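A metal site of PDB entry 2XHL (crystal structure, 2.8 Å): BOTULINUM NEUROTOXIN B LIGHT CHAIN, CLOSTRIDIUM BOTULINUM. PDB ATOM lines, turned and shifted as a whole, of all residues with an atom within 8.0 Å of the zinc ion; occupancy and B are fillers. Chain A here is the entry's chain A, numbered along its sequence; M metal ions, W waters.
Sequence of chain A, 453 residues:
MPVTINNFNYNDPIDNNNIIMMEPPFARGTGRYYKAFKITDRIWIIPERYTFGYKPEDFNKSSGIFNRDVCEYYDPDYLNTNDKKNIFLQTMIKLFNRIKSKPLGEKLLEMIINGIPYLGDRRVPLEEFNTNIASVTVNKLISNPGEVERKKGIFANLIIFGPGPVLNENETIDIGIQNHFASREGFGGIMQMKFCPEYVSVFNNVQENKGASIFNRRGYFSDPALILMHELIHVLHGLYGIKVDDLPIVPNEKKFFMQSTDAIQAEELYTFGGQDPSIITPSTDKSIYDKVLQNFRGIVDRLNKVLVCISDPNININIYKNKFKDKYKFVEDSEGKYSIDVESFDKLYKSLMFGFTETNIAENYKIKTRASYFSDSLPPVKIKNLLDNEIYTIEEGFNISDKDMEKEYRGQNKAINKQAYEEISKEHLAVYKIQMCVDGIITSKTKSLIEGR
ND1 of His 234 is in hydrogen-bond range of OE2 of Glu 267, at 3.0 Å.
A ring nitrogen (ND1) of His 230 sits at hydrogen-bond distance from the side-chain carboxylate (OE1) of Glu 358.
Three residues have an atom within 4 Å of the zinc ion: His 230, His 234 and Glu 268.
The nearest printed residue that does not touch the zinc ion is Glu 231 (4.5 Å).
The zinc ion is bound by water W1 (2.1 Å), NE2 of His 234 (2.2 Å), NE2 of His 230 (2.3 Å), OE2 of Glu 268 (2.3 Å) and OE1 of Glu 268 (2.5 Å).
The zinc ion has five donor atoms within binding distance.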
ATOM      1  N   ASN A 170      -2.698  21.150 -35.101  1.00  0.00           N
ATOM      2  CA  ASN A 170      -2.365  21.248 -33.677  1.00  0.00           C
ATOM      3  C   ASN A 170      -3.551  20.884 -32.784  1.00  0.00           C
ATOM      4  O   ASN A 170      -4.606  21.510 -32.858  1.00  0.00           O
ATOM      5  CB  ASN A 170      -1.850  22.655 -33.353  1.00  0.00           C
ATOM      6  CG  ASN A 170      -0.610  23.021 -34.147  1.00  0.00           C
ATOM      7  OD1 ASN A 170       0.285  22.185 -34.378  1.00  0.00           O
ATOM      8  ND2 ASN A 170      -0.533  24.276 -34.576  1.00  0.00           N
ATOM      9  N   GLU A 171      -3.355  19.867 -31.949  1.00  0.00           N
ATOM     10  CA  GLU A 171      -4.434  19.341 -31.112  1.00  0.00           C
ATOM     11  C   GLU A 171      -4.020  19.225 -29.651  1.00  0.00           C
ATOM     12  O   GLU A 171      -2.852  18.994 -29.339  1.00  0.00           O
ATOM     13  CB  GLU A 171      -4.895  17.971 -31.621  1.00  0.00           C
ATOM     14  CG  GLU A 171      -6.331  17.623 -31.224  1.00  0.00           C
ATOM     15  CD  GLU A 171      -6.663  16.141 -31.359  1.00  0.00           C
ATOM     16  OE1 GLU A 171      -6.016  15.427 -32.159  1.00  0.00           O
ATOM     17  OE2 GLU A 171      -7.607  15.695 -30.663  1.00  0.00           O
ATOM     18  N   THR A 172      -4.997  19.389 -28.764  1.00  0.00           N
ATOM     19  CA  THR A 172      -4.790  19.199 -27.341  1.00  0.00           C
ATOM     20  C   THR A 172      -5.609  18.006 -26.881  1.00  0.00           C
ATOM     21  O   THR A 172      -6.834  18.054 -26.853  1.00  0.00           O
ATOM     22  CB  THR A 172      -5.180  20.457 -26.554  1.00  0.00           C
ATOM     23  OG1 THR A 172      -4.457  21.593 -27.058  1.00  0.00           O
ATOM     24  CG2 THR A 172      -4.879  20.274 -25.066  1.00  0.00           C
ATOM     25  N   ILE A 227      -1.922  30.760 -32.164  1.00  0.00           N
ATOM     26  CA  ILE A 227      -2.207  29.342 -32.373  1.00  0.00           C
ATOM     27  C   ILE A 227      -1.858  28.525 -31.128  1.00  0.00           C
ATOM     28  O   ILE A 227      -2.580  27.597 -30.762  1.00  0.00           O
ATOM     29  CB  ILE A 227      -1.417  28.793 -33.607  1.00  0.00           C
ATOM     30  CG1 ILE A 227      -1.897  29.457 -34.903  1.00  0.00           C
ATOM     31  CG2 ILE A 227      -1.540  27.271 -33.725  1.00  0.00           C
ATOM     32  CD1 ILE A 227      -0.921  29.331 -36.051  1.00  0.00           C
ATOM     33  N   HIS A 230      -4.420  29.541 -28.404  1.00  0.00           N
ATOM     34  CA  HIS A 230      -5.662  28.848 -28.680  1.00  0.00           C
ATOM     35  C   HIS A 230      -5.629  27.492 -28.011  1.00  0.00           C
ATOM     36  O   HIS A 230      -6.551  27.137 -27.279  1.00  0.00           O
ATOM     37  CB  HIS A 230      -5.884  28.696 -30.188  1.00  0.00           C
ATOM     38  CG  HIS A 230      -7.090  27.882 -30.548  1.00  0.00           C
ATOM     39  ND1 HIS A 230      -8.307  28.449 -30.846  1.00  0.00           N
ATOM     40  CD2 HIS A 230      -7.263  26.542 -30.645  1.00  0.00           C
ATOM     41  CE1 HIS A 230      -9.183  27.490 -31.125  1.00  0.00           C
ATOM     42  NE2 HIS A 230      -8.572  26.324 -31.013  1.00  0.00           N
ATOM     43  N   GLU A 231      -4.548  26.751 -28.243  1.00  0.00           N
ATOM     44  CA  GLU A 231      -4.388  25.413 -27.665  1.00  0.00           C
ATOM     45  C   GLU A 231      -4.276  25.449 -26.142  1.00  0.00           C
ATOM     46  O   GLU A 231      -4.772  24.544 -25.468  1.00  0.00           O
ATOM     47  CB  GLU A 231      -3.183  24.691 -28.269  1.00  0.00           C
ATOM     48  CG  GLU A 231      -3.263  24.421 -29.784  1.00  0.00           C
ATOM     49  CD  GLU A 231      -4.523  23.667 -30.226  1.00  0.00           C
ATOM     50  OE1 GLU A 231      -5.011  22.773 -29.478  1.00  0.00           O
ATOM     51  OE2 GLU A 231      -5.026  23.951 -31.334  1.00  0.00           O
ATOM     52  N   ILE A 233      -5.754  27.459 -24.113  1.00  0.00           N
ATOM     53  CA  ILE A 233      -7.115  27.604 -23.594  1.00  0.00           C
ATOM     54  C   ILE A 233      -7.768  26.224 -23.427  1.00  0.00           C
ATOM     55  O   ILE A 233      -8.396  25.955 -22.401  1.00  0.00           O
ATOM     56  CB  ILE A 233      -7.978  28.510 -24.510  1.00  0.00           C
ATOM     57  CG1 ILE A 233      -7.399  29.923 -24.552  1.00  0.00           C
ATOM     58  CG2 ILE A 233      -9.420  28.555 -24.030  1.00  0.00           C
ATOM     59  CD1 ILE A 233      -7.809  30.736 -25.777  1.00  0.00           C
ATOM     60  N   HIS A 234      -7.608  25.363 -24.427  1.00  0.00           N
ATOM     61  CA  HIS A 234      -8.075  23.977 -24.330  1.00  0.00           C
ATOM     62  C   HIS A 234      -7.436  23.303 -23.122  1.00  0.00           C
ATOM     63  O   HIS A 234      -8.112  22.619 -22.355  1.00  0.00           O
ATOM     64  CB  HIS A 234      -7.758  23.187 -25.604  1.00  0.00           C
ATOM     65  CG  HIS A 234      -8.667  23.510 -26.755  1.00  0.00           C
ATOM     66  ND1 HIS A 234     -10.043  23.449 -26.671  1.00  0.00           N
ATOM     67  CD2 HIS A 234      -8.385  23.880 -28.030  1.00  0.00           C
ATOM     68  CE1 HIS A 234     -10.563  23.774 -27.829  1.00  0.00           C
ATOM     69  NE2 HIS A 234      -9.590  24.044 -28.671  1.00  0.00           N
ATOM     70  N   LYS A 243     -13.868  20.648 -19.727  1.00  0.00           N
ATOM     71  CA  LYS A 243     -13.992  20.348 -21.141  1.00  0.00           C
ATOM     72  C   LYS A 243     -15.081  19.280 -21.319  1.00  0.00           C
ATOM     73  O   LYS A 243     -14.795  18.165 -21.766  1.00  0.00           O
ATOM     74  CB  LYS A 243     -12.645  19.860 -21.699  1.00  0.00           C
ATOM     75  CG  LYS A 243     -12.596  19.692 -23.222  1.00  0.00           C
ATOM     76  CD  LYS A 243     -11.204  19.251 -23.672  1.00  0.00           C
ATOM     77  CE  LYS A 243     -11.236  18.704 -25.129  1.00  0.00           C
ATOM     78  NZ  LYS A 243      -9.862  18.290 -25.582  1.00  0.00           N
ATOM     79  N   GLU A 267     -17.433  23.474 -26.520  1.00  0.00           N
ATOM     80  CA  GLU A 267     -16.141  23.834 -25.954  1.00  0.00           C
ATOM     81  C   GLU A 267     -15.187  24.415 -27.011  1.00  0.00           C
ATOM     82  O   GLU A 267     -14.443  25.352 -26.732  1.00  0.00           O
ATOM     83  CB  GLU A 267     -15.533  22.628 -25.236  1.00  0.00           C
ATOM     84  CG  GLU A 267     -14.367  22.944 -24.310  1.00  0.00           C
ATOM     85  CD  GLU A 267     -13.028  22.906 -25.017  1.00  0.00           C
ATOM     86  OE1 GLU A 267     -12.947  22.319 -26.116  1.00  0.00           O
ATOM     87  OE2 GLU A 267     -12.057  23.468 -24.471  1.00  0.00           O
ATOM     88  N   GLU A 268     -15.233  23.859 -28.218  1.00  0.00           N
ATOM     89  CA  GLU A 268     -14.422  24.345 -29.334  1.00  0.00           C
ATOM     90  C   GLU A 268     -14.904  25.713 -29.820  1.00  0.00           C
ATOM     91  O   GLU A 268     -14.102  26.561 -30.232  1.00  0.00           O
ATOM     92  CB  GLU A 268     -14.417  23.323 -30.481  1.00  0.00           C
ATOM     93  CG  GLU A 268     -13.596  23.721 -31.725  1.00  0.00           C
ATOM     94  CD  GLU A 268     -12.090  23.818 -31.467  1.00  0.00           C
ATOM     95  OE1 GLU A 268     -11.452  22.767 -31.208  1.00  0.00           O
ATOM     96  OE2 GLU A 268     -11.552  24.947 -31.549  1.00  0.00           O
ATOM     97  N   LEU A 269     -16.208  25.952 -29.751  1.00  0.00           N
ATOM     98  CA  LEU A 269     -16.789  27.227 -30.175  1.00  0.00           C
ATOM     99  C   LEU A 269     -16.659  28.326 -29.113  1.00  0.00           C
ATOM    100  O   LEU A 269     -16.537  29.499 -29.461  1.00  0.00           O
ATOM    101  CB  LEU A 269     -18.250  27.050 -30.618  1.00  0.00           C
ATOM    102  CG  LEU A 269     -18.492  26.263 -31.901  1.00  0.00           C
ATOM    103  CD1 LEU A 269     -19.984  26.122 -32.154  1.00  0.00           C
ATOM    104  CD2 LEU A 269     -17.808  26.888 -33.119  1.00  0.00           C
ATOM    105  N   THR A 271     -14.045  28.404 -27.058  1.00  0.00           N
ATOM    106  CA  THR A 271     -12.607  28.657 -27.143  1.00  0.00           C
ATOM    107  C   THR A 271     -12.257  29.653 -28.259  1.00  0.00           C
ATOM    108  O   THR A 271     -11.441  30.551 -28.041  1.00  0.00           O
ATOM    109  CB  THR A 271     -11.810  27.336 -27.282  1.00  0.00           C
ATOM    110  OG1 THR A 271     -11.914  26.604 -26.055  1.00  0.00           O
ATOM    111  CG2 THR A 271     -10.348  27.592 -27.574  1.00  0.00           C
ATOM    112  N   PHE A 272     -12.879  29.496 -29.426  1.00  0.00           N
ATOM    113  CA  PHE A 272     -12.709  30.460 -30.511  1.00  0.00           C
ATOM    114  C   PHE A 272     -13.258  31.822 -30.107  1.00  0.00           C
ATOM    115  O   PHE A 272     -12.607  32.850 -30.293  1.00  0.00           O
ATOM    116  CB  PHE A 272     -13.375  29.974 -31.806  1.00  0.00           C
ATOM    117  CG  PHE A 272     -13.070  30.846 -32.999  1.00  0.00           C
ATOM    118  CD1 PHE A 272     -11.950  30.612 -33.782  1.00  0.00           C
ATOM    119  CD2 PHE A 272     -13.906  31.910 -33.333  1.00  0.00           C
ATOM    120  CE1 PHE A 272     -11.658  31.413 -34.876  1.00  0.00           C
ATOM    121  CE2 PHE A 272     -13.620  32.720 -34.425  1.00  0.00           C
ATOM    122  CZ  PHE A 272     -12.497  32.460 -35.207  1.00  0.00           C
ATOM    123  N   GLU A 358      -9.725  32.977 -28.257  1.00  0.00           N
ATOM    124  CA  GLU A 358      -8.831  33.353 -29.353  1.00  0.00           C
ATOM    125  C   GLU A 358      -9.130  34.761 -29.889  1.00  0.00           C
ATOM    126  O   GLU A 358      -8.208  35.519 -30.199  1.00  0.00           O
ATOM    127  CB  GLU A 358      -8.899  32.324 -30.506  1.00  0.00           C
ATOM    128  CG  GLU A 358      -7.926  32.594 -31.659  1.00  0.00           C
ATOM    129  CD  GLU A 358      -7.951  31.511 -32.740  1.00  0.00           C
ATOM    130  OE1 GLU A 358      -7.963  30.311 -32.386  1.00  0.00           O
ATOM    131  OE2 GLU A 358      -7.962  31.850 -33.947  1.00  0.00           O
ATOM    132  N   TYR A 373     -15.142  30.228 -36.932  1.00  0.00           N
ATOM    133  CA  TYR A 373     -14.624  28.858 -36.954  1.00  0.00           C
ATOM    134  C   TYR A 373     -14.981  28.180 -38.296  1.00  0.00           C
ATOM    135  O   TYR A 373     -14.251  27.300 -38.767  1.00  0.00           O
ATOM    136  CB  TYR A 373     -15.170  28.051 -35.774  1.00  0.00           C
ATOM    137  CG  TYR A 373     -14.889  26.561 -35.816  1.00  0.00           C
ATOM    138  CD1 TYR A 373     -13.743  26.031 -35.222  1.00  0.00           C
ATOM    139  CD2 TYR A 373     -15.770  25.693 -36.445  1.00  0.00           C
ATOM    140  CE1 TYR A 373     -13.483  24.657 -35.258  1.00  0.00           C
ATOM    141  CE2 TYR A 373     -15.521  24.317 -36.507  1.00  0.00           C
ATOM    142  CZ  TYR A 373     -14.387  23.814 -35.902  1.00  0.00           C
ATOM    143  OH  TYR A 373     -14.143  22.458 -35.956  1.00  0.00           O
HETATM  144 ZN    ZN M   1      -9.475  24.222 -30.858  1.00  0.00          ZN
HETATM  145  O   HOH W   1      -7.887  23.403 -32.043  1.00  0.00           O
